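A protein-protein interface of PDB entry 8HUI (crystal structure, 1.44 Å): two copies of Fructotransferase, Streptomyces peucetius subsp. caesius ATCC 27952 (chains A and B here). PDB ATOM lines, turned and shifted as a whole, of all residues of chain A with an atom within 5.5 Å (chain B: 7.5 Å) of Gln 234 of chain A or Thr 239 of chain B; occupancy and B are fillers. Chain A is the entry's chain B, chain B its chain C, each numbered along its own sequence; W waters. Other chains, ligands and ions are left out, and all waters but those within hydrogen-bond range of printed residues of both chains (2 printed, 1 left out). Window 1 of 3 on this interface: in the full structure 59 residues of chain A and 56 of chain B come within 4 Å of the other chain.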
ATOM      1  N   VAL A 208      11.328  19.401  24.721  1.00  0.00           N
ATOM      2  CA  VAL A 208      11.363  20.846  24.917  1.00  0.00           C
ATOM      3  C   VAL A 208      10.023  21.530  24.685  1.00  0.00           C
ATOM      4  O   VAL A 208       9.939  22.584  24.043  1.00  0.00           O
ATOM      5  CB  VAL A 208      12.516  21.494  24.131  1.00  0.00           C
ATOM      6  CG1 VAL A 208      13.834  20.967  24.676  1.00  0.00           C
ATOM      7  CG2 VAL A 208      12.425  21.210  22.619  1.00  0.00           C
ATOM      8  N   ALA A 209       8.978  20.977  25.261  1.00  0.00           N
ATOM      9  CA  ALA A 209       7.713  21.680  25.292  1.00  0.00           C
ATOM     10  C   ALA A 209       7.827  22.948  26.141  1.00  0.00           C
ATOM     11  O   ALA A 209       8.534  22.976  27.154  1.00  0.00           O
ATOM     12  CB  ALA A 209       6.631  20.747  25.838  1.00  0.00           C
ATOM     13  N   LYS A 210       7.117  23.997  25.730  1.00  0.00           N
ATOM     14  CA  LYS A 210       7.056  25.245  26.474  1.00  0.00           C
ATOM     15  C   LYS A 210       5.611  25.504  26.862  1.00  0.00           C
ATOM     16  O   LYS A 210       4.759  25.690  25.991  1.00  0.00           O
ATOM     17  CB  LYS A 210       7.604  26.396  25.626  1.00  0.00           C
ATOM     18  CG  LYS A 210       7.559  27.778  26.326  1.00  0.00           C
ATOM     19  CD  LYS A 210       8.622  28.731  25.800  1.00  0.00           C
ATOM     20  CE  LYS A 210       8.404  29.098  24.343  1.00  0.00           C
ATOM     21  NZ  LYS A 210       7.167  29.946  24.036  1.00  0.00           N
ATOM     22  N   ILE A 211       5.343  25.528  28.162  1.00  0.00           N
ATOM     23  CA  ILE A 211       4.003  25.733  28.711  1.00  0.00           C
ATOM     24  C   ILE A 211       4.084  26.958  29.604  1.00  0.00           C
ATOM     25  O   ILE A 211       4.597  26.884  30.729  1.00  0.00           O
ATOM     26  CB  ILE A 211       3.493  24.509  29.482  1.00  0.00           C
ATOM     27  CG1 ILE A 211       3.435  23.293  28.555  1.00  0.00           C
ATOM     28  CG2 ILE A 211       2.105  24.769  30.081  1.00  0.00           C
ATOM     29  CD1 ILE A 211       3.088  21.985  29.289  1.00  0.00           C
ATOM     30  N   THR A 212       3.590  28.096  29.104  1.00  0.00           N
ATOM     31  CA  THR A 212       3.788  29.374  29.771  1.00  0.00           C
ATOM     32  C   THR A 212       2.520  30.207  29.799  1.00  0.00           C
ATOM     33  O   THR A 212       1.707  30.199  28.870  1.00  0.00           O
ATOM     34  CB  THR A 212       4.885  30.173  29.064  1.00  0.00           C
ATOM     35  OG1 THR A 212       4.544  30.289  27.677  1.00  0.00           O
ATOM     36  CG2 THR A 212       6.228  29.483  29.193  1.00  0.00           C
ATOM     37  N   GLY A 232      13.215  17.981  28.876  1.00  0.00           N
ATOM     38  CA  GLY A 232      13.392  19.423  28.768  1.00  0.00           C
ATOM     39  C   GLY A 232      12.138  20.274  28.793  1.00  0.00           C
ATOM     40  O   GLY A 232      12.144  21.386  28.247  1.00  0.00           O
ATOM     41  N   LEU A 233      11.078  19.799  29.423  1.00  0.00           N
ATOM     42  CA  LEU A 233       9.846  20.571  29.536  1.00  0.00           C
ATOM     43  C   LEU A 233      10.107  21.846  30.310  1.00  0.00           C
ATOM     44  O   LEU A 233      10.808  21.830  31.315  1.00  0.00           O
ATOM     45  CB  LEU A 233       8.858  19.682  30.293  1.00  0.00           C
ATOM     46  CG  LEU A 233       7.444  20.096  30.634  1.00  0.00           C
ATOM     47  CD1 LEU A 233       6.657  20.523  29.420  1.00  0.00           C
ATOM     48  CD2 LEU A 233       6.790  18.898  31.335  1.00  0.00           C
ATOM     49  N   GLN A 234       9.566  22.968  29.825  1.00  0.00           N
ATOM     50  CA  GLN A 234       9.626  24.226  30.545  1.00  0.00           C
ATOM     51  C   GLN A 234       8.198  24.578  30.904  1.00  0.00           C
ATOM     52  O   GLN A 234       7.346  24.683  30.012  1.00  0.00           O
ATOM     53  CB  GLN A 234      10.233  25.377  29.743  1.00  0.00           C
ATOM     54  CG  GLN A 234      10.378  26.549  30.727  1.00  0.00           C
ATOM     55  CD  GLN A 234      10.394  27.924  30.162  1.00  0.00           C
ATOM     56  OE1 GLN A 234      10.358  28.868  30.938  1.00  0.00           O
ATOM     57  NE2 GLN A 234      10.468  28.077  28.841  1.00  0.00           N
ATOM     58  N   ILE A 235       7.943  24.780  32.191  1.00  0.00           N
ATOM     59  CA  ILE A 235       6.627  25.161  32.713  1.00  0.00           C
ATOM     60  C   ILE A 235       6.836  26.393  33.576  1.00  0.00           C
ATOM     61  O   ILE A 235       7.416  26.292  34.669  1.00  0.00           O
ATOM     62  CB  ILE A 235       5.998  24.033  33.545  1.00  0.00           C
ATOM     63  CG1 ILE A 235       5.786  22.765  32.713  1.00  0.00           C
ATOM     64  CG2 ILE A 235       4.687  24.495  34.178  1.00  0.00           C
ATOM     65  CD1 ILE A 235       5.486  21.529  33.558  1.00  0.00           C
ATOM     66  N   SER A 236       6.368  27.554  33.108  1.00  0.00           N
ATOM     67  CA  SER A 236       6.628  28.788  33.844  1.00  0.00           C
ATOM     68  C   SER A 236       5.549  29.832  33.592  1.00  0.00           C
ATOM     69  O   SER A 236       4.923  29.881  32.537  1.00  0.00           O
ATOM     70  CB  SER A 236       8.016  29.339  33.519  1.00  0.00           C
ATOM     71  OG  SER A 236       8.118  29.696  32.147  1.00  0.00           O
ATOM     72  N   ALA A 254      13.453  18.937  33.258  1.00  0.00           N
ATOM     73  CA  ALA A 254      12.393  19.931  33.238  1.00  0.00           C
ATOM     74  C   ALA A 254      12.773  21.144  34.087  1.00  0.00           C
ATOM     75  O   ALA A 254      13.539  21.061  35.049  1.00  0.00           O
ATOM     76  CB  ALA A 254      11.074  19.364  33.788  1.00  0.00           C
ATOM     77  N   SER A 255      12.198  22.284  33.722  1.00  0.00           N
ATOM     78  CA  SER A 255      12.370  23.548  34.427  1.00  0.00           C
ATOM     79  C   SER A 255      10.974  24.042  34.777  1.00  0.00           C
ATOM     80  O   SER A 255      10.229  24.472  33.894  1.00  0.00           O
ATOM     81  CB  SER A 255      13.096  24.556  33.543  1.00  0.00           C
ATOM     82  OG  SER A 255      13.513  25.641  34.331  1.00  0.00           O
ATOM     83  N   THR A 257       9.231  26.623  37.019  1.00  0.00           N
ATOM     84  CA  THR A 257       9.653  27.812  37.730  1.00  0.00           C
ATOM     85  C   THR A 257       8.618  28.914  37.593  1.00  0.00           C
ATOM     86  O   THR A 257       7.889  29.002  36.602  1.00  0.00           O
ATOM     87  CB  THR A 257      10.999  28.333  37.170  1.00  0.00           C
ATOM     88  OG1 THR A 257      10.848  28.664  35.773  1.00  0.00           O
ATOM     89  CG2 THR A 257      12.085  27.300  37.301  1.00  0.00           C
ATOM     90  N   ASN B 191       8.609  34.217  20.160  1.00  0.00           N
ATOM     91  CA  ASN B 191       9.165  33.893  18.855  1.00  0.00           C
ATOM     92  C   ASN B 191       9.744  32.485  18.827  1.00  0.00           C
ATOM     93  O   ASN B 191       9.945  31.830  19.852  1.00  0.00           O
ATOM     94  CB  ASN B 191      10.263  34.899  18.497  1.00  0.00           C
ATOM     95  CG  ASN B 191       9.747  36.306  18.464  1.00  0.00           C
ATOM     96  OD1 ASN B 191       8.960  36.654  17.586  1.00  0.00           O
ATOM     97  ND2 ASN B 191      10.206  37.140  19.384  1.00  0.00           N
ATOM     98  N   ILE B 193      12.962  31.039  16.968  1.00  0.00           N
ATOM     99  CA  ILE B 193      14.185  31.332  16.229  1.00  0.00           C
ATOM    100  C   ILE B 193      15.036  30.076  16.284  1.00  0.00           C
ATOM    101  O   ILE B 193      15.448  29.648  17.366  1.00  0.00           O
ATOM    102  CB  ILE B 193      14.938  32.530  16.815  1.00  0.00           C
ATOM    103  CG1 ILE B 193      14.063  33.789  16.739  1.00  0.00           C
ATOM    104  CG2 ILE B 193      16.266  32.734  16.042  1.00  0.00           C
ATOM    105  CD1 ILE B 193      14.622  35.002  17.479  1.00  0.00           C
ATOM    106  N   THR B 212      11.318  37.456  26.381  1.00  0.00           N
ATOM    107  CA  THR B 212      10.494  36.522  27.151  1.00  0.00           C
ATOM    108  C   THR B 212       9.819  35.489  26.262  1.00  0.00           C
ATOM    109  O   THR B 212       9.419  35.775  25.129  1.00  0.00           O
ATOM    110  CB  THR B 212       9.390  37.244  27.939  1.00  0.00           C
ATOM    111  OG1 THR B 212       8.643  38.042  27.016  1.00  0.00           O
ATOM    112  CG2 THR B 212       9.949  38.139  29.046  1.00  0.00           C
ATOM    113  N   ASN B 213       9.655  34.279  26.812  1.00  0.00           N
ATOM    114  CA  ASN B 213       8.746  33.302  26.224  1.00  0.00           C
ATOM    115  C   ASN B 213       9.118  32.923  24.786  1.00  0.00           C
ATOM    116  O   ASN B 213       8.248  32.606  23.984  1.00  0.00           O
ATOM    117  CB  ASN B 213       7.297  33.817  26.288  1.00  0.00           C
ATOM    118  CG  ASN B 213       6.278  32.751  25.970  1.00  0.00           C
ATOM    119  OD1 ASN B 213       6.483  31.570  26.257  1.00  0.00           O
ATOM    120  ND2 ASN B 213       5.142  33.159  25.421  1.00  0.00           N
ATOM    121  N   ASN B 214      10.415  32.869  24.480  1.00  0.00           N
ATOM    122  CA  ASN B 214      10.882  32.514  23.146  1.00  0.00           C
ATOM    123  C   ASN B 214      11.487  31.115  23.124  1.00  0.00           C
ATOM    124  O   ASN B 214      12.003  30.628  24.130  1.00  0.00           O
ATOM    125  CB  ASN B 214      11.998  33.465  22.675  1.00  0.00           C
ATOM    126  CG  ASN B 214      11.569  34.920  22.576  1.00  0.00           C
ATOM    127  OD1 ASN B 214      10.821  35.311  21.668  1.00  0.00           O
ATOM    128  ND2 ASN B 214      12.058  35.739  23.499  1.00  0.00           N
ATOM    129  N   PHE B 215      11.465  30.499  21.939  1.00  0.00           N
ATOM    130  CA  PHE B 215      12.394  29.432  21.592  1.00  0.00           C
ATOM    131  C   PHE B 215      13.571  30.068  20.860  1.00  0.00           C
ATOM    132  O   PHE B 215      13.373  30.748  19.846  1.00  0.00           O
ATOM    133  CB  PHE B 215      11.730  28.428  20.659  1.00  0.00           C
ATOM    134  CG  PHE B 215      10.880  27.410  21.342  1.00  0.00           C
ATOM    135  CD1 PHE B 215      11.465  26.350  22.033  1.00  0.00           C
ATOM    136  CD2 PHE B 215       9.508  27.452  21.250  1.00  0.00           C
ATOM    137  CE1 PHE B 215      10.682  25.380  22.646  1.00  0.00           C
ATOM    138  CE2 PHE B 215       8.727  26.466  21.846  1.00  0.00           C
ATOM    139  CZ  PHE B 215       9.323  25.445  22.543  1.00  0.00           C
ATOM    140  N   LEU B 216      14.782  29.888  21.389  1.00  0.00           N
ATOM    141  CA  LEU B 216      16.015  30.372  20.766  1.00  0.00           C
ATOM    142  C   LEU B 216      16.955  29.200  20.555  1.00  0.00           C
ATOM    143  O   LEU B 216      17.437  28.602  21.523  1.00  0.00           O
ATOM    144  CB  LEU B 216      16.700  31.440  21.615  1.00  0.00           C
ATOM    145  CG  LEU B 216      15.814  32.596  22.070  1.00  0.00           C
ATOM    146  CD1 LEU B 216      16.564  33.542  22.995  1.00  0.00           C
ATOM    147  CD2 LEU B 216      15.277  33.354  20.886  1.00  0.00           C
ATOM    148  N   ILE B 217      17.192  28.873  19.294  1.00  0.00           N
ATOM    149  CA  ILE B 217      17.826  27.619  18.899  1.00  0.00           C
ATOM    150  C   ILE B 217      18.894  27.874  17.853  1.00  0.00           C
ATOM    151  O   ILE B 217      18.916  27.220  16.798  1.00  0.00           O
ATOM    152  CB  ILE B 217      16.818  26.550  18.473  1.00  0.00           C
ATOM    153  CG1 ILE B 217      15.601  26.542  19.396  1.00  0.00           C
ATOM    154  CG2 ILE B 217      17.491  25.181  18.506  1.00  0.00           C
ATOM    155  CD1 ILE B 217      14.547  25.503  19.054  1.00  0.00           C
ATOM    156  N   SER B 236      13.552  36.018  30.519  1.00  0.00           N
ATOM    157  CA  SER B 236      12.796  35.096  31.359  1.00  0.00           C
ATOM    158  C   SER B 236      11.798  34.274  30.551  1.00  0.00           C
ATOM    159  O   SER B 236      11.271  34.720  29.532  1.00  0.00           O
ATOM    160  CB  SER B 236      12.098  35.827  32.506  1.00  0.00           C
ATOM    161  OG  SER B 236      11.103  36.669  32.009  1.00  0.00           O
ATOM    162  N   GLY B 237      11.565  33.043  31.009  1.00  0.00           N
ATOM    163  CA  GLY B 237      10.593  32.169  30.398  1.00  0.00           C
ATOM    164  C   GLY B 237      10.958  31.674  29.026  1.00  0.00           C
ATOM    165  O   GLY B 237      10.095  31.194  28.293  1.00  0.00           O
ATOM    166  N   ASN B 238      12.231  31.724  28.667  1.00  0.00           N
ATOM    167  CA  ASN B 238      12.671  31.258  27.365  1.00  0.00           C
ATOM    168  C   ASN B 238      13.138  29.824  27.458  1.00  0.00           C
ATOM    169  O   ASN B 238      13.619  29.365  28.502  1.00  0.00           O
ATOM    170  CB  ASN B 238      13.837  32.102  26.864  1.00  0.00           C
ATOM    171  CG  ASN B 238      13.476  33.537  26.747  1.00  0.00           C
ATOM    172  OD1 ASN B 238      12.762  33.934  25.810  1.00  0.00           O
ATOM    173  ND2 ASN B 238      13.953  34.353  27.694  1.00  0.00           N
ATOM    174  N   THR B 239      13.016  29.130  26.343  1.00  0.00           N
ATOM    175  CA  THR B 239      13.669  27.843  26.112  1.00  0.00           C
ATOM    176  C   THR B 239      14.770  28.085  25.095  1.00  0.00           C
ATOM    177  O   THR B 239      14.497  28.376  23.924  1.00  0.00           O
ATOM    178  CB  THR B 239      12.652  26.818  25.637  1.00  0.00           C
ATOM    179  OG1 THR B 239      11.763  26.528  26.727  1.00  0.00           O
ATOM    180  CG2 THR B 239      13.342  25.517  25.224  1.00  0.00           C
ATOM    181  N   ILE B 240      16.013  27.970  25.550  1.00  0.00           N
ATOM    182  CA  ILE B 240      17.190  28.284  24.752  1.00  0.00           C
ATOM    183  C   ILE B 240      18.016  27.015  24.627  1.00  0.00           C
ATOM    184  O   ILE B 240      18.481  26.466  25.634  1.00  0.00           O
ATOM    185  CB  ILE B 240      17.995  29.414  25.396  1.00  0.00           C
ATOM    186  CG1 ILE B 240      17.061  30.595  25.709  1.00  0.00           C
ATOM    187  CG2 ILE B 240      19.135  29.831  24.470  1.00  0.00           C
ATOM    188  CD1 ILE B 240      17.802  31.875  26.238  1.00  0.00           C
ATOM    189  N   LEU B 241      18.224  26.569  23.394  1.00  0.00           N
ATOM    190  CA  LEU B 241      18.633  25.203  23.105  1.00  0.00           C
ATOM    191  C   LEU B 241      19.810  25.177  22.135  1.00  0.00           C
ATOM    192  O   LEU B 241      20.207  26.198  21.548  1.00  0.00           O
ATOM    193  CB  LEU B 241      17.479  24.424  22.500  1.00  0.00           C
ATOM    194  CG  LEU B 241      16.211  24.364  23.345  1.00  0.00           C
ATOM    195  CD1 LEU B 241      15.162  23.657  22.537  1.00  0.00           C
ATOM    196  CD2 LEU B 241      16.455  23.684  24.672  1.00  0.00           C
ATOM    197  N   CYS B 244      22.963  27.272  23.563  1.00  0.00           N
ATOM    198  CA  CYS B 244      22.597  28.392  24.418  1.00  0.00           C
ATOM    199  C   CYS B 244      23.836  29.179  24.782  1.00  0.00           C
ATOM    200  O   CYS B 244      24.762  28.638  25.386  1.00  0.00           O
ATOM    201  CB  CYS B 244      21.971  27.886  25.713  1.00  0.00           C
ATOM    202  SG  CYS B 244      21.639  29.226  26.938  1.00  0.00           S
ATOM    203  N   THR B 257      16.093  34.911  34.602  1.00  0.00           N
ATOM    204  CA  THR B 257      15.344  34.109  35.550  1.00  0.00           C
ATOM    205  C   THR B 257      14.367  33.195  34.829  1.00  0.00           C
ATOM    206  O   THR B 257      13.845  33.521  33.765  1.00  0.00           O
ATOM    207  CB  THR B 257      14.571  35.014  36.535  1.00  0.00           C
ATOM    208  OG1 THR B 257      13.699  35.892  35.811  1.00  0.00           O
ATOM    209  CG2 THR B 257      15.518  35.872  37.354  1.00  0.00           C
ATOM    210  N   SER B 258      14.113  32.030  35.428  1.00  0.00           N
ATOM    211  CA  SER B 258      13.017  31.184  34.975  1.00  0.00           C
ATOM    212  C   SER B 258      13.149  30.804  33.504  1.00  0.00           C
ATOM    213  O   SER B 258      12.164  30.803  32.756  1.00  0.00           O
ATOM    214  CB  SER B 258      11.691  31.901  35.268  1.00  0.00           C
ATOM    215  OG  SER B 258      10.552  31.158  34.888  1.00  0.00           O
ATOM    216  N   ASN B 259      14.361  30.421  33.090  1.00  0.00           N
ATOM    217  CA  ASN B 259      14.594  29.938  31.742  1.00  0.00           C
ATOM    218  C   ASN B 259      15.067  28.494  31.770  1.00  0.00           C
ATOM    219  O   ASN B 259      15.684  28.047  32.735  1.00  0.00           O
ATOM    220  CB  ASN B 259      15.695  30.714  31.023  1.00  0.00           C
ATOM    221  CG  ASN B 259      15.419  32.189  30.937  1.00  0.00           C
ATOM    222  OD1 ASN B 259      14.646  32.643  30.081  1.00  0.00           O
ATOM    223  ND2 ASN B 259      16.078  32.965  31.789  1.00  0.00           N
ATOM    224  N   LYS B 260      14.779  27.805  30.677  1.00  0.00           N
ATOM    225  CA  LYS B 260      15.320  26.483  30.363  1.00  0.00           C
ATOM    226  C   LYS B 260      16.477  26.695  29.395  1.00  0.00           C
ATOM    227  O   LYS B 260      16.268  27.178  28.275  1.00  0.00           O
ATOM    228  CB  LYS B 260      14.207  25.647  29.743  1.00  0.00           C
ATOM    229  CG  LYS B 260      14.641  24.462  28.924  1.00  0.00           C
ATOM    230  CD  LYS B 260      15.117  23.353  29.769  1.00  0.00           C
ATOM    231  CE  LYS B 260      15.608  22.233  28.838  1.00  0.00           C
ATOM    232  NZ  LYS B 260      16.250  21.212  29.656  1.00  0.00           N
ATOM    233  N   LEU B 261      17.694  26.338  29.824  1.00  0.00           N
ATOM    234  CA  LEU B 261      18.910  26.680  29.095  1.00  0.00           C
ATOM    235  C   LEU B 261      19.725  25.424  28.808  1.00  0.00           C
ATOM    236  O   LEU B 261      20.081  24.690  29.736  1.00  0.00           O
ATOM    237  CB  LEU B 261      19.764  27.651  29.898  1.00  0.00           C
ATOM    238  CG  LEU B 261      19.078  28.904  30.443  1.00  0.00           C
ATOM    239  CD1 LEU B 261      19.994  29.662  31.405  1.00  0.00           C
ATOM    240  CD2 LEU B 261      18.660  29.784  29.295  1.00  0.00           C
ATOM    241  N   LEU B 262      20.036  25.179  27.537  1.00  0.00           N
ATOM    242  CA  LEU B 262      20.707  23.943  27.135  1.00  0.00           C
ATOM    243  C   LEU B 262      21.746  24.245  26.068  1.00  0.00           C
ATOM    244  O   LEU B 262      21.472  24.968  25.103  1.00  0.00           O
ATOM    245  CB  LEU B 262      19.701  22.918  26.608  1.00  0.00           C
ATOM    246  CG  LEU B 262      20.350  21.564  26.258  1.00  0.00           C
ATOM    247  CD1 LEU B 262      19.374  20.439  26.534  1.00  0.00           C
ATOM    248  CD2 LEU B 262      20.828  21.488  24.835  1.00  0.00           C
ATOM    249  N   ALA B 282      16.819  30.757  39.371  1.00  0.00           N
ATOM    250  CA  ALA B 282      15.716  29.851  39.030  1.00  0.00           C
ATOM    251  C   ALA B 282      15.731  29.460  37.550  1.00  0.00           C
ATOM    252  O   ALA B 282      14.704  29.476  36.881  1.00  0.00           O
ATOM    253  CB  ALA B 282      14.352  30.433  39.447  1.00  0.00           C
HETATM  254  O   HOH W   1       7.587  30.574  21.233  1.00  0.00           O
HETATM  255  O   HOH W   2      12.042  27.777  33.371  1.00  0.00           O
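Printed residues of chain B within 4 Å of Gln 234 of chain A: Gly 237 (3.2 Å), Asn 238 (3.4 Å), Thr 239 (2.9 Å), Ser 258 (3.2 Å) and Lys 260 (3.98 Å). Printed residues of chain A within 4 Å of Asn 238 of chain B: Gln 234. Printed residues of chain B within 4 Å of Val 208 of chain A: Phe 215 (3.2 Å) and Leu 241 (3.7 Å). Of the printed residues of chain B, Lys 210 of chain A touches Asn 213 (2.8 Å), Asn 214 (3.9 Å), Phe 215 (3.6 Å), Gly 237 (3.8 Å) and Thr 239 (3.9 Å). The nearest printed residue of chain B that does not touch Thr 257 of chain A is Asn 259 of chain B (4.8 Å).
Water W2 lies within hydrogen-bond range of the side-chain hydroxyl (OG) of Ser 255 of chain A, the side-chain hydroxyl (OG1) of Thr 257 of chain A, the backbone carbonyl oxygen (O) of Ser 258 of chain B and the side-chain amide oxygen (OE1) of Gln 234 of chain A. Water W1 lies within hydrogen-bond range of NZ of Lys 210 of chain A (2.9 Å), O of Asn 191 of chain B (3.0 Å) and O of Asn 213 of chain B (3.5 Å).
Positions printed for both chains: 212, 236 and 257.
NE2 of Gln 234 of chain A is in hydrogen-bond range of O of Gly 237 of chain B (3.2 Å). The side-chain amide nitrogen of Gln 234 of chain A sits at hydrogen-bond distance from the backbone carbonyl oxygen of Asn 238 of chain B (3.4 Å). The side-chain hydroxyl (OG1) of Thr 239 of chain B is in hydrogen-bond range of the side-chain amide nitrogen (NE2) of Gln 234 of chain A (2.9 Å). OG1 of Thr 212 of chain A is in hydrogen-bond range of OD1 of Asn 213 of chain B (2.7 Å). The side-chain amide oxygen (OD1) of Asn 213 of chain B sits at hydrogen-bond distance from the side-chain amino group (NZ) of Lys 210 of chain A (2.8 Å). The side-chain amide oxygen (OE1) of Gln 234 of chain A sits close to the backbone carbonyl oxygen (O) of Ser 258 of chain B. The side-chain hydroxyl of Thr 257 of chain A is in hydrogen-bond range of the side-chain hydroxyl of Ser 258 of chain B, 2.7 Å away.
N of Asn 213 of chain B lies close to O of Gly 237 of chain B (3.5 Å). The backbone NH (N) of Leu 241 of chain B lies within hydrogen-bond range of the backbone carbonyl oxygen (O) of Leu 216 of chain B, 2.9 Å away. The backbone NH (N) of Ser 258 of chain B lies within hydrogen-bond range of the backbone carbonyl oxygen (O) of Ala 282 of chain B (3.0 Å). N of Ile 211 of chain A lies within hydrogen-bond range of O of Gln 234 of chain A (2.9 Å). The backbone carbonyl oxygen (O) of Phe 215 of chain B sits at hydrogen-bond distance from the backbone NH (N) of Ile 193 of chain B, at 2.9 Å. The side-chain amide oxygen (OD1) of Asn 259 of chain B is in hydrogen-bond range of the backbone NH (N) of Asn 238 of chain B.
Val 208 of chain A touches Phe 215 of chain B. Val 208 of chain A touches Leu 241 of chain B (CG2 to CD1, 3.7 Å). Lys 210 of chain A touches Asn 214 of chain B (CE to C, 3.9 Å). Phe 215 of chain B touches Lys 210 of chain A. Thr 239 of chain B touches Lys 210 of chain A (OG1 to CD, 3.9 Å). Gly 232 of chain A touches Lys 260 of chain B. Gln 234 of chain A touches Lys 260 of chain B. Ser 236 of chain A touches Ser 258 of chain B (CB to OG, 3.4 Å). Asn 259 of chain B touches Ser 255 of chain A. Thr 257 of chain A touches Ala 282 of chain B.
Printed residues of chain A that touch a printed residue of chain B: Val 208, Lys 210, Thr 212, Gly 232, Gln 234, Ser 236, Ser 255 and Thr 257. Of the 22 printed residues of chain B, 11 touch a printed residue of chain A. Printed residues of chain B that touch a printed residue of chain A: Asn 213, Asn 214, Phe 215, Gly 237, Asn 238, Thr 239, Leu 241, Ser 258, Asn 259, Lys 260 and Ala 282.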
